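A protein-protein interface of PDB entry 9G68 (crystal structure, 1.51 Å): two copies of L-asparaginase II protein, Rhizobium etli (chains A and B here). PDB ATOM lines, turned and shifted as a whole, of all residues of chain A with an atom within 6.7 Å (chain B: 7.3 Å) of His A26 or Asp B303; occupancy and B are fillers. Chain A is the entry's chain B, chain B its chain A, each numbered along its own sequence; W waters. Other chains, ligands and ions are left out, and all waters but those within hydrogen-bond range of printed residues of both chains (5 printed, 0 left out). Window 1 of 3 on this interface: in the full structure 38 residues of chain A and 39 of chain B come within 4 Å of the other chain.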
ATOM      1  N   ASP A  12       4.305   1.597  11.528  1.00  0.00           N
ATOM      2  CA  ASP A  12       3.622   1.369  12.809  1.00  0.00           C
ATOM      3  C   ASP A  12       2.246   2.034  12.756  1.00  0.00           C
ATOM      4  O   ASP A  12       2.125   3.250  12.941  1.00  0.00           O
ATOM      5  CB  ASP A  12       4.454   1.884  13.972  1.00  0.00           C
ATOM      6  CG  ASP A  12       5.638   0.962  14.314  1.00  0.00           C
ATOM      7  OD1 ASP A  12       5.549  -0.263  14.079  1.00  0.00           O
ATOM      8  OD2 ASP A  12       6.647   1.476  14.851  1.00  0.00           O
ATOM      9  N   PHE A  13       1.205   1.220  12.516  1.00  0.00           N
ATOM     10  CA  PHE A  13      -0.146   1.717  12.305  1.00  0.00           C
ATOM     11  C   PHE A  13      -1.142   1.048  13.241  1.00  0.00           C
ATOM     12  O   PHE A  13      -0.971  -0.107  13.655  1.00  0.00           O
ATOM     13  CB  PHE A  13      -0.643   1.429  10.853  1.00  0.00           C
ATOM     14  CG  PHE A  13      -0.090   2.334   9.825  1.00  0.00           C
ATOM     15  CD1 PHE A  13      -0.697   3.544   9.581  1.00  0.00           C
ATOM     16  CD2 PHE A  13       1.023   1.956   9.066  1.00  0.00           C
ATOM     17  CE1 PHE A  13      -0.224   4.388   8.586  1.00  0.00           C
ATOM     18  CE2 PHE A  13       1.513   2.805   8.083  1.00  0.00           C
ATOM     19  CZ  PHE A  13       0.870   4.030   7.849  1.00  0.00           C
ATOM     20  N   VAL A  14      -2.227   1.778  13.518  1.00  0.00           N
ATOM     21  CA  VAL A  14      -3.480   1.175  13.947  1.00  0.00           C
ATOM     22  C   VAL A  14      -4.483   1.405  12.813  1.00  0.00           C
ATOM     23  O   VAL A  14      -4.483   2.468  12.178  1.00  0.00           O
ATOM     24  CB  VAL A  14      -3.967   1.738  15.311  1.00  0.00           C
ATOM     25  CG1 VAL A  14      -4.150   3.272  15.305  1.00  0.00           C
ATOM     26  CG2 VAL A  14      -5.239   0.982  15.755  1.00  0.00           C
ATOM     27  N   VAL A  15      -5.276   0.372  12.513  1.00  0.00           N
ATOM     28  CA  VAL A  15      -6.068   0.316  11.287  1.00  0.00           C
ATOM     29  C   VAL A  15      -7.473  -0.129  11.641  1.00  0.00           C
ATOM     30  O   VAL A  15      -7.639  -1.046  12.449  1.00  0.00           O
ATOM     31  CB  VAL A  15      -5.435  -0.659  10.277  1.00  0.00           C
ATOM     32  CG1 VAL A  15      -6.318  -0.828   9.060  1.00  0.00           C
ATOM     33  CG2 VAL A  15      -3.994  -0.205   9.904  1.00  0.00           C
ATOM     34  N   THR A  16      -8.489   0.496  11.038  1.00  0.00           N
ATOM     35  CA  THR A  16      -9.846  -0.038  11.126  1.00  0.00           C
ATOM     36  C   THR A  16     -10.231  -0.636   9.783  1.00  0.00           C
ATOM     37  O   THR A  16      -9.790  -0.151   8.731  1.00  0.00           O
ATOM     38  CB  THR A  16     -10.850   1.045  11.530  1.00  0.00           C
ATOM     39  OG1 THR A  16     -10.735   2.131  10.621  1.00  0.00           O
ATOM     40  CG2 THR A  16     -10.527   1.570  12.935  1.00  0.00           C
ATOM     41  N   GLU A  23     -10.437   0.669   6.109  1.00  0.00           N
ATOM     42  CA  GLU A  23     -11.182   1.922   6.192  1.00  0.00           C
ATOM     43  C   GLU A  23     -10.215   3.085   6.405  1.00  0.00           C
ATOM     44  O   GLU A  23      -9.905   3.806   5.451  1.00  0.00           O
ATOM     45  CB  GLU A  23     -12.229   1.811   7.309  1.00  0.00           C
ATOM     46  CG  GLU A  23     -13.144   2.993   7.417  1.00  0.00           C
ATOM     47  CD  GLU A  23     -14.459   2.789   6.684  1.00  0.00           C
ATOM     48  OE1 GLU A  23     -15.254   1.912   7.132  1.00  0.00           O
ATOM     49  OE2 GLU A  23     -14.699   3.459   5.639  1.00  0.00           O
ATOM     50  N   ASN A  24      -9.710   3.248   7.631  1.00  0.00           N
ATOM     51  CA  ASN A  24      -8.736   4.282   7.999  1.00  0.00           C
ATOM     52  C   ASN A  24      -7.467   3.651   8.547  1.00  0.00           C
ATOM     53  O   ASN A  24      -7.498   2.555   9.107  1.00  0.00           O
ATOM     54  CB  ASN A  24      -9.277   5.207   9.085  1.00  0.00           C
ATOM     55  CG  ASN A  24     -10.621   5.796   8.728  1.00  0.00           C
ATOM     56  OD1 ASN A  24     -10.874   6.155   7.580  1.00  0.00           O
ATOM     57  ND2 ASN A  24     -11.483   5.934   9.738  1.00  0.00           N
ATOM     58  N   SER A  25      -6.344   4.351   8.404  1.00  0.00           N
ATOM     59  CA  SER A  25      -5.142   3.953   9.123  1.00  0.00           C
ATOM     60  C   SER A  25      -4.555   5.176   9.788  1.00  0.00           C
ATOM     61  O   SER A  25      -4.727   6.315   9.320  1.00  0.00           O
ATOM     62  CB  SER A  25      -4.114   3.274   8.210  1.00  0.00           C
ATOM     63  OG  SER A  25      -3.641   4.131   7.209  1.00  0.00           O
ATOM     64  N   HIS A  26      -3.861   4.921  10.894  1.00  0.00           N
ATOM     65  CA  HIS A  26      -3.393   5.987  11.783  1.00  0.00           C
ATOM     66  C   HIS A  26      -1.971   5.652  12.208  1.00  0.00           C
ATOM     67  O   HIS A  26      -1.713   4.546  12.694  1.00  0.00           O
ATOM     68  CB  HIS A  26      -4.265   6.069  13.039  1.00  0.00           C
ATOM     69  CG  HIS A  26      -5.734   6.129  12.758  1.00  0.00           C
ATOM     70  ND1 HIS A  26      -6.434   7.317  12.800  1.00  0.00           N
ATOM     71  CD2 HIS A  26      -6.639   5.168  12.461  1.00  0.00           C
ATOM     72  CE1 HIS A  26      -7.707   7.089  12.531  1.00  0.00           C
ATOM     73  NE2 HIS A  26      -7.861   5.792  12.326  1.00  0.00           N
ATOM     74  N   ARG A  27      -1.062   6.579  12.005  1.00  0.00           N
ATOM     75  CA  ARG A  27       0.307   6.354  12.438  1.00  0.00           C
ATOM     76  C   ARG A  27       0.443   6.500  13.955  1.00  0.00           C
ATOM     77  O   ARG A  27      -0.110   7.436  14.562  1.00  0.00           O
ATOM     78  CB  ARG A  27       1.234   7.342  11.735  1.00  0.00           C
ATOM     79  CG  ARG A  27       1.697   6.884  10.359  1.00  0.00           C
ATOM     80  CD  ARG A  27       2.470   5.540  10.375  1.00  0.00           C
ATOM     81  NE  ARG A  27       3.372   5.468  11.535  1.00  0.00           N
ATOM     82  CZ  ARG A  27       4.488   6.178  11.687  1.00  0.00           C
ATOM     83  NH1 ARG A  27       4.974   6.927  10.709  1.00  0.00           N
ATOM     84  NH2 ARG A  27       5.107   6.163  12.860  1.00  0.00           N
ATOM     85  N   VAL A  28       1.247   5.619  14.551  1.00  0.00           N
ATOM     86  CA  VAL A  28       1.493   5.558  15.993  1.00  0.00           C
ATOM     87  C   VAL A  28       2.940   5.944  16.305  1.00  0.00           C
ATOM     88  O   VAL A  28       3.869   5.488  15.626  1.00  0.00           O
ATOM     89  CB  VAL A  28       1.189   4.141  16.536  1.00  0.00           C
ATOM     90  CG1 VAL A  28       1.508   4.083  18.036  1.00  0.00           C
ATOM     91  CG2 VAL A  28      -0.275   3.784  16.265  1.00  0.00           C
ATOM     92  N   ILE A 301      -0.922   9.668  18.536  1.00  0.00           N
ATOM     93  CA  ILE A 301      -1.520   9.255  17.270  1.00  0.00           C
ATOM     94  C   ILE A 301      -1.360  10.430  16.314  1.00  0.00           C
ATOM     95  O   ILE A 301      -1.790  11.550  16.621  1.00  0.00           O
ATOM     96  CB  ILE A 301      -3.008   8.891  17.420  1.00  0.00           C
ATOM     97  CG1 ILE A 301      -3.229   7.834  18.520  1.00  0.00           C
ATOM     98  CG2 ILE A 301      -3.550   8.495  16.031  1.00  0.00           C
ATOM     99  CD1 ILE A 301      -2.487   6.540  18.211  1.00  0.00           C
ATOM    100  N   GLU A 302      -0.661  10.220  15.206  1.00  0.00           N
ATOM    101  CA  GLU A 302      -0.208  11.366  14.406  1.00  0.00           C
ATOM    102  C   GLU A 302      -1.358  12.266  13.951  1.00  0.00           C
ATOM    103  O   GLU A 302      -1.211  13.496  13.879  1.00  0.00           O
ATOM    104  CB  GLU A 302       0.582  10.855  13.197  1.00  0.00           C
ATOM    105  CG  GLU A 302       1.061  11.934  12.223  1.00  0.00           C
ATOM    106  CD  GLU A 302       2.110  12.830  12.842  1.00  0.00           C
ATOM    107  OE1 GLU A 302       2.904  12.333  13.684  1.00  0.00           O
ATOM    108  OE2 GLU A 302       2.140  14.051  12.532  1.00  0.00           O
ATOM    109  N   ASP A 303      -2.496  11.686  13.617  1.00  0.00           N
ATOM    110  CA  ASP A 303      -3.639  12.421  13.080  1.00  0.00           C
ATOM    111  C   ASP A 303      -4.600  12.884  14.180  1.00  0.00           C
ATOM    112  O   ASP A 303      -5.616  13.501  13.864  1.00  0.00           O
ATOM    113  CB  ASP A 303      -4.398  11.542  12.089  1.00  0.00           C
ATOM    114  CG  ASP A 303      -4.769  10.210  12.716  1.00  0.00           C
ATOM    115  OD1 ASP A 303      -5.848  10.122  13.371  1.00  0.00           O
ATOM    116  OD2 ASP A 303      -3.941   9.266  12.625  1.00  0.00           O
ATOM    117  N   GLY A 304      -4.346  12.540  15.432  1.00  0.00           N
ATOM    118  CA  GLY A 304      -5.124  13.049  16.570  1.00  0.00           C
ATOM    119  C   GLY A 304      -6.397  12.294  16.934  1.00  0.00           C
ATOM    120  O   GLY A 304      -7.218  12.831  17.689  1.00  0.00           O
ATOM    121  N   ASN A 305      -6.596  11.070  16.449  1.00  0.00           N
ATOM    122  CA  ASN A 305      -7.831  10.336  16.729  1.00  0.00           C
ATOM    123  C   ASN A 305      -7.795   9.729  18.144  1.00  0.00           C
ATOM    124  O   ASN A 305      -6.958   8.872  18.444  1.00  0.00           O
ATOM    125  CB  ASN A 305      -8.054   9.245  15.683  1.00  0.00           C
ATOM    126  CG  ASN A 305      -9.376   8.592  15.840  1.00  0.00           C
ATOM    127  OD1 ASN A 305      -9.606   7.918  16.830  1.00  0.00           O
ATOM    128  ND2 ASN A 305     -10.283   8.815  14.889  1.00  0.00           N
ATOM    129  N   MET A 308      -8.689   5.849  18.606  1.00  0.00           N
ATOM    130  CA  MET A 308      -7.527   5.018  18.295  1.00  0.00           C
ATOM    131  C   MET A 308      -6.447   5.108  19.379  1.00  0.00           C
ATOM    132  O   MET A 308      -5.781   4.103  19.684  1.00  0.00           O
ATOM    133  CB  MET A 308      -6.956   5.436  16.930  1.00  0.00           C
ATOM    134  CG  MET A 308      -7.930   5.211  15.727  1.00  0.00           C
ATOM    135  SD  MET A 308      -8.331   3.456  15.526  1.00  0.00           S
ATOM    136  CE  MET A 308      -9.886   3.225  16.368  1.00  0.00           C
ATOM    137  N   VAL A 312      -4.812   1.899  21.179  1.00  0.00           N
ATOM    138  CA  VAL A 312      -3.363   1.669  21.087  1.00  0.00           C
ATOM    139  C   VAL A 312      -2.713   1.599  22.472  1.00  0.00           C
ATOM    140  O   VAL A 312      -1.850   0.749  22.723  1.00  0.00           O
ATOM    141  CB  VAL A 312      -2.713   2.757  20.216  1.00  0.00           C
ATOM    142  CG1 VAL A 312      -1.178   2.758  20.417  1.00  0.00           C
ATOM    143  CG2 VAL A 312      -3.091   2.604  18.766  1.00  0.00           C
ATOM    144  N   PHE B  13       0.310  15.845   2.573  1.00  0.00           N
ATOM    145  CA  PHE B  13      -0.292  15.997   3.885  1.00  0.00           C
ATOM    146  C   PHE B  13      -1.039  17.311   3.999  1.00  0.00           C
ATOM    147  O   PHE B  13      -0.682  18.309   3.367  1.00  0.00           O
ATOM    148  CB  PHE B  13       0.781  15.961   5.018  1.00  0.00           C
ATOM    149  CG  PHE B  13       1.350  14.597   5.232  1.00  0.00           C
ATOM    150  CD1 PHE B  13       2.369  14.118   4.428  1.00  0.00           C
ATOM    151  CD2 PHE B  13       0.804  13.766   6.208  1.00  0.00           C
ATOM    152  CE1 PHE B  13       2.874  12.821   4.611  1.00  0.00           C
ATOM    153  CE2 PHE B  13       1.296  12.482   6.405  1.00  0.00           C
ATOM    154  CZ  PHE B  13       2.326  12.000   5.605  1.00  0.00           C
ATOM    155  N   VAL B  14      -2.096  17.302   4.816  1.00  0.00           N
ATOM    156  CA  VAL B  14      -2.609  18.524   5.419  1.00  0.00           C
ATOM    157  C   VAL B  14      -2.178  18.521   6.892  1.00  0.00           C
ATOM    158  O   VAL B  14      -2.206  17.487   7.563  1.00  0.00           O
ATOM    159  CB  VAL B  14      -4.146  18.652   5.234  1.00  0.00           C
ATOM    160  CG1 VAL B  14      -4.865  17.383   5.652  1.00  0.00           C
ATOM    161  CG2 VAL B  14      -4.666  19.886   5.994  1.00  0.00           C
ATOM    162  N   SER B  25      -1.036  15.689  11.632  1.00  0.00           N
ATOM    163  CA  SER B  25      -0.942  15.665  10.190  1.00  0.00           C
ATOM    164  C   SER B  25      -1.782  14.512   9.657  1.00  0.00           C
ATOM    165  O   SER B  25      -1.999  13.493  10.339  1.00  0.00           O
ATOM    166  CB  SER B  25       0.513  15.569   9.737  1.00  0.00           C
ATOM    167  OG  SER B  25       1.089  14.314  10.089  1.00  0.00           O
ATOM    168  N   HIS B  26      -2.242  14.701   8.425  1.00  0.00           N
ATOM    169  CA  HIS B  26      -3.223  13.831   7.780  1.00  0.00           C
ATOM    170  C   HIS B  26      -2.777  13.566   6.348  1.00  0.00           C
ATOM    171  O   HIS B  26      -2.569  14.503   5.563  1.00  0.00           O
ATOM    172  CB  HIS B  26      -4.619  14.499   7.785  1.00  0.00           C
ATOM    173  CG  HIS B  26      -5.044  15.012   9.127  1.00  0.00           C
ATOM    174  ND1 HIS B  26      -5.925  14.326   9.931  1.00  0.00           N
ATOM    175  CD2 HIS B  26      -4.735  16.156   9.797  1.00  0.00           C
ATOM    176  CE1 HIS B  26      -6.130  15.017  11.045  1.00  0.00           C
ATOM    177  NE2 HIS B  26      -5.424  16.129  10.990  1.00  0.00           N
ATOM    178  N   ARG B  27      -2.661  12.293   5.990  1.00  0.00           N
ATOM    179  CA  ARG B  27      -2.269  11.930   4.642  1.00  0.00           C
ATOM    180  C   ARG B  27      -3.454  12.084   3.687  1.00  0.00           C
ATOM    181  O   ARG B  27      -4.584  11.689   4.010  1.00  0.00           O
ATOM    182  CB  ARG B  27      -1.740  10.498   4.639  1.00  0.00           C
ATOM    183  CG  ARG B  27      -1.255  10.042   3.272  1.00  0.00           C
ATOM    184  CD  ARG B  27      -0.699   8.609   3.325  1.00  0.00           C
ATOM    185  NE  ARG B  27       0.537   8.501   4.094  1.00  0.00           N
ATOM    186  CZ  ARG B  27       1.740   8.780   3.608  1.00  0.00           C
ATOM    187  NH1 ARG B  27       1.900   9.242   2.372  1.00  0.00           N
ATOM    188  NH2 ARG B  27       2.805   8.597   4.376  1.00  0.00           N
ATOM    189  N   VAL B  28      -3.209  12.686   2.529  1.00  0.00           N
ATOM    190  CA  VAL B  28      -4.242  13.020   1.547  1.00  0.00           C
ATOM    191  C   VAL B  28      -4.014  12.191   0.292  1.00  0.00           C
ATOM    192  O   VAL B  28      -2.878  12.117  -0.218  1.00  0.00           O
ATOM    193  CB  VAL B  28      -4.227  14.518   1.178  1.00  0.00           C
ATOM    194  CG1 VAL B  28      -5.284  14.811   0.115  1.00  0.00           C
ATOM    195  CG2 VAL B  28      -4.435  15.393   2.386  1.00  0.00           C
ATOM    196  N   HIS B  29      -5.086  11.572  -0.212  1.00  0.00           N
ATOM    197  CA  HIS B  29      -5.123  10.922  -1.517  1.00  0.00           C
ATOM    198  C   HIS B  29      -6.181  11.585  -2.379  1.00  0.00           C
ATOM    199  O   HIS B  29      -7.269  11.915  -1.899  1.00  0.00           O
ATOM    200  CB  HIS B  29      -5.450   9.437  -1.399  1.00  0.00           C
ATOM    201  CG  HIS B  29      -4.595   8.721  -0.412  1.00  0.00           C
ATOM    202  ND1 HIS B  29      -3.326   8.287  -0.718  1.00  0.00           N
ATOM    203  CD2 HIS B  29      -4.827   8.354   0.871  1.00  0.00           C
ATOM    204  CE1 HIS B  29      -2.821   7.651   0.329  1.00  0.00           C
ATOM    205  NE2 HIS B  29      -3.699   7.713   1.321  1.00  0.00           N
ATOM    206  N   ARG B  48      -5.658   4.240  -4.524  1.00  0.00           N
ATOM    207  CA  ARG B  48      -5.903   3.614  -3.226  1.00  0.00           C
ATOM    208  C   ARG B  48      -7.228   2.866  -3.202  1.00  0.00           C
ATOM    209  O   ARG B  48      -8.276   3.433  -3.530  1.00  0.00           O
ATOM    210  CB  ARG B  48      -5.913   4.690  -2.133  1.00  0.00           C
ATOM    211  CG  ARG B  48      -6.149   4.108  -0.725  1.00  0.00           C
ATOM    212  CD  ARG B  48      -6.534   5.240   0.241  1.00  0.00           C
ATOM    213  NE  ARG B  48      -6.579   4.849   1.660  1.00  0.00           N
ATOM    214  CZ  ARG B  48      -7.660   4.356   2.251  1.00  0.00           C
ATOM    215  NH1 ARG B  48      -8.800   4.168   1.576  1.00  0.00           N
ATOM    216  NH2 ARG B  48      -7.599   4.042   3.553  1.00  0.00           N
ATOM    217  N   ASP B 273     -16.216   8.412   6.853  1.00  0.00           N
ATOM    218  CA  ASP B 273     -14.783   8.215   7.062  1.00  0.00           C
ATOM    219  C   ASP B 273     -13.969   8.949   6.001  1.00  0.00           C
ATOM    220  O   ASP B 273     -12.830   8.580   5.694  1.00  0.00           O
ATOM    221  CB  ASP B 273     -14.436   6.721   7.169  1.00  0.00           C
ATOM    222  CG  ASP B 273     -14.935   6.134   8.500  1.00  0.00           C
ATOM    223  OD1 ASP B 273     -14.506   6.661   9.550  1.00  0.00           O
ATOM    224  OD2 ASP B 273     -15.795   5.229   8.500  1.00  0.00           O
ATOM    225  N   ALA B 274     -14.518  10.084   5.551  1.00  0.00           N
ATOM    226  CA  ALA B 274     -13.739  11.173   4.920  1.00  0.00           C
ATOM    227  C   ALA B 274     -13.290  10.826   3.492  1.00  0.00           C
ATOM    228  O   ALA B 274     -12.112  10.985   3.129  1.00  0.00           O
ATOM    229  CB  ALA B 274     -12.542  11.596   5.792  1.00  0.00           C
ATOM    230  N   LYS B 300      -9.616  11.116  -0.435  1.00  0.00           N
ATOM    231  CA  LYS B 300      -9.715  10.340   0.805  1.00  0.00           C
ATOM    232  C   LYS B 300      -8.661  10.851   1.779  1.00  0.00           C
ATOM    233  O   LYS B 300      -7.481  10.969   1.418  1.00  0.00           O
ATOM    234  CB  LYS B 300      -9.514   8.826   0.525  1.00  0.00           C
ATOM    235  CG  LYS B 300      -9.225   7.941   1.751  1.00  0.00           C
ATOM    236  CD  LYS B 300     -10.413   7.794   2.713  1.00  0.00           C
ATOM    237  CE  LYS B 300     -10.020   6.883   3.893  1.00  0.00           C
ATOM    238  NZ  LYS B 300     -11.164   6.666   4.829  1.00  0.00           N
ATOM    239  N   ILE B 301      -9.083  11.201   2.992  1.00  0.00           N
ATOM    240  CA  ILE B 301      -8.153  11.513   4.078  1.00  0.00           C
ATOM    241  C   ILE B 301      -7.855  10.185   4.766  1.00  0.00           C
ATOM    242  O   ILE B 301      -8.779   9.507   5.258  1.00  0.00           O
ATOM    243  CB  ILE B 301      -8.742  12.519   5.076  1.00  0.00           C
ATOM    244  CG1 ILE B 301      -9.121  13.849   4.393  1.00  0.00           C
ATOM    245  CG2 ILE B 301      -7.753  12.765   6.260  1.00  0.00           C
ATOM    246  CD1 ILE B 301      -7.946  14.488   3.664  1.00  0.00           C
ATOM    247  N   GLU B 302      -6.578   9.775   4.767  1.00  0.00           N
ATOM    248  CA  GLU B 302      -6.241   8.407   5.185  1.00  0.00           C
ATOM    249  C   GLU B 302      -6.766   8.038   6.578  1.00  0.00           C
ATOM    250  O   GLU B 302      -7.193   6.903   6.820  1.00  0.00           O
ATOM    251  CB  GLU B 302      -4.729   8.198   5.171  1.00  0.00           C
ATOM    252  CG  GLU B 302      -4.352   6.763   5.583  1.00  0.00           C
ATOM    253  CD  GLU B 302      -4.808   5.697   4.560  1.00  0.00           C
ATOM    254  OE1 GLU B 302      -4.888   6.009   3.343  1.00  0.00           O
ATOM    255  OE2 GLU B 302      -5.096   4.541   4.953  1.00  0.00           O
ATOM    256  N   ASP B 303      -6.707   8.959   7.511  1.00  0.00           N
ATOM    257  CA  ASP B 303      -7.101   8.689   8.890  1.00  0.00           C
ATOM    258  C   ASP B 303      -8.585   8.981   9.135  1.00  0.00           C
ATOM    259  O   ASP B 303      -9.080   8.755  10.254  1.00  0.00           O
ATOM    260  CB  ASP B 303      -6.262   9.547   9.840  1.00  0.00           C
ATOM    261  CG  ASP B 303      -6.351  11.009   9.459  1.00  0.00           C
ATOM    262  OD1 ASP B 303      -7.318  11.696   9.878  1.00  0.00           O
ATOM    263  OD2 ASP B 303      -5.531  11.451   8.634  1.00  0.00           O
ATOM    264  N   GLY B 304      -9.293   9.523   8.154  1.00  0.00           N
ATOM    265  CA  GLY B 304     -10.744   9.642   8.254  1.00  0.00           C
ATOM    266  C   GLY B 304     -11.274  10.922   8.858  1.00  0.00           C
ATOM    267  O   GLY B 304     -12.461  10.974   9.210  1.00  0.00           O
ATOM    268  N   ASN B 305     -10.455  11.962   8.971  1.00  0.00           N
ATOM    269  CA  ASN B 305     -10.874  13.213   9.607  1.00  0.00           C
ATOM    270  C   ASN B 305     -11.706  14.069   8.636  1.00  0.00           C
ATOM    271  O   ASN B 305     -11.211  14.532   7.595  1.00  0.00           O
ATOM    272  CB  ASN B 305      -9.643  13.972  10.091  1.00  0.00           C
ATOM    273  CG  ASN B 305     -10.007  15.196  10.902  1.00  0.00           C
ATOM    274  OD1 ASN B 305     -10.563  16.152  10.373  1.00  0.00           O
ATOM    275  ND2 ASN B 305      -9.689  15.166  12.196  1.00  0.00           N
ATOM    276  N   LEU B 306     -12.951  14.331   8.993  1.00  0.00           N
ATOM    277  CA  LEU B 306     -13.851  15.065   8.100  1.00  0.00           C
ATOM    278  C   LEU B 306     -13.491  16.548   7.995  1.00  0.00           C
ATOM    279  O   LEU B 306     -13.624  17.151   6.927  1.00  0.00           O
ATOM    280  CB  LEU B 306     -15.285  14.954   8.602  1.00  0.00           C
ATOM    281  CG  LEU B 306     -15.994  13.604   8.599  1.00  0.00           C
ATOM    282  CD1 LEU B 306     -17.362  13.820   9.189  1.00  0.00           C
ATOM    283  CD2 LEU B 306     -16.119  13.106   7.185  1.00  0.00           C
ATOM    284  N   MET B 308     -10.666  17.915   8.090  1.00  0.00           N
ATOM    285  CA  MET B 308      -9.538  18.032   7.181  1.00  0.00           C
ATOM    286  C   MET B 308      -9.967  17.759   5.763  1.00  0.00           C
ATOM    287  O   MET B 308      -9.463  18.417   4.842  1.00  0.00           O
ATOM    288  CB  MET B 308      -8.410  17.089   7.605  1.00  0.00           C
ATOM    289  CG  MET B 308      -7.733  17.472   8.927  1.00  0.00           C
ATOM    290  SD  MET B 308      -6.945  19.096   8.917  1.00  0.00           S
ATOM    291  CE  MET B 308      -8.272  20.139   9.531  1.00  0.00           C
HETATM  292  O   HOH W   1     -10.348  10.162  12.370  1.00  0.00           O
HETATM  293  O   HOH W   2     -11.216   2.893   2.658  1.00  0.00           O
HETATM  294  O   HOH W   3     -13.041   4.619   3.977  1.00  0.00           O
HETATM  295  O   HOH W   4      -8.134  11.348  12.466  1.00  0.00           O
HETATM  296  O   HOH W   5      -8.268  13.496  13.971  1.00  0.00           O
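OE2 of Glu A302 lies within hydrogen-bond range of OG of Ser B25, 2.7 Å away.
The guanidinium group of Arg B48 is in hydrogen-bond range of the backbone carbonyl oxygen of Glu A23.
ND2 of Asn A24 lies within hydrogen-bond range of OD1 of Asp B273 (3.1 Å).
The side-chain amino group of Lys B300 lies within hydrogen-bond range of the backbone carbonyl oxygen of Glu A23.
The side-chain amide oxygen of Asn A24 lies within hydrogen-bond range of the side-chain amino group of Lys B300 (2.8 Å).
The side-chain carboxylate of Glu B302 is in hydrogen-bond range of the side-chain hydroxyl of Ser A25 (2.7 Å).
O of Val B14 lies within hydrogen-bond range of N of His B26 (2.9 Å).
The backbone carbonyl oxygen (O) of Arg B27 lies within hydrogen-bond range of the backbone NH (N) of Glu B302 (2.9 Å).
OD1 of Asp B303 sits close to N of Asn B305 (3.3 Å).
O of Val A14 lies within hydrogen-bond range of N of His A26, 2.8 Å away.
The backbone carbonyl oxygen (O) of Thr A16 is in hydrogen-bond range of the backbone NH (N) of Glu A23 (2.8 Å).
The backbone NH (N) of Thr A16 lies within hydrogen-bond range of the backbone carbonyl oxygen (O) of Asn A24, 3.0 Å away.
Among the printed residues, pairs that only touch across the chains: His A26 with Asp B303 (3.1 Å), Asp A303 with His B26 (3.2 Å), Asn A24 with Glu B302 (3.3 Å), Asp A303 with Asp B303 (3.3 Å), Glu A23 with Asp B273 (3.3 Å), Asp A303 with Ser B25 (3.4 Å), Ser A25 with Asp B303 (3.4 Å), Asn A24 with Gly B304 (3.6 Å) and Asn A24 with Asp B303 (3.7 Å).
Of chain B, only Asp B303 (3.1 Å) comes within 4 Å of His A26.
Asp B303 touches four residues of chain A.
Of the printed residues of chain A, Asp B273 touches Glu A23 and Asn A24.
Of the printed residues of chain A, Glu B302 touches Asn A24 (3.3 Å) and Ser A25 (2.7 Å).
Ile B301 touches none of the printed residues of chain A.
Phe B13 touches none of the printed residues of chain A.
The nearest residue of chain B that does not touch His A26 is Gly B304 (5.3 Å).
The nearest printed residue of chain A that does not touch Glu B302 is Glu A23 (4.3 Å).
Of the 18 printed residues of chain B, 8 touch a printed residue of chain A.
Printed residues of chain B that touch a printed residue of chain A: Ser B25, His B26, Arg B48, Asp B273, Lys B300, Glu B302, Asp B303 and Gly B304.
Printed residues of chain A that touch a printed residue of chain B: Glu A23, Asn A24, Ser A25, His A26, Glu A302 and Asp A303.
Hydrophobic or aromatic side chains of chain A that line the printed part of chain B: His A26.
Among the printed residues, no Asp or Glu carboxylate lies within 4 Å of a Lys or Arg side-chain nitrogen of the other chain.
Ser A25 touches Glu B302, and with the chains exchanged Glu A302 touches Ser B25.
Ser A25 touches Asp B303, and with the chains exchanged Asp A303 touches Ser B25.
His A26 touches Asp B303, and with the chains exchanged Asp A303 touches His B26.
Asp B303 touches its own counterpart, Asp A303.
Of the 15 pairs that touch across the chains among the printed residues, 7 have their exchanged pair printed and touching as well.
Water W3 bridges the side-chain carboxylate of Glu A23 (2.6 Å) and the side-chain amino group of Lys B300 (2.9 Å).
Water W5 lies within hydrogen-bond range of the backbone carbonyl oxygen of Asp A303 (2.7 Å) and the side-chain amide nitrogen of Asn B305 (2.8 Å).
Water W4 lies within hydrogen-bond range of the side-chain carboxylate of Asp B303 and the side-chain carboxylate of Asp A303.
Water W1 lies within hydrogen-bond range of the backbone carbonyl oxygen (O) of Asp B303 and the side-chain amide nitrogen (ND2) of Asn A305.
Water W2 lies within hydrogen-bond range of the guanidinium group (NH1) of Arg B48 (2.9 Å) and the backbone carbonyl oxygen (O) of Glu A23 (3.2 Å).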
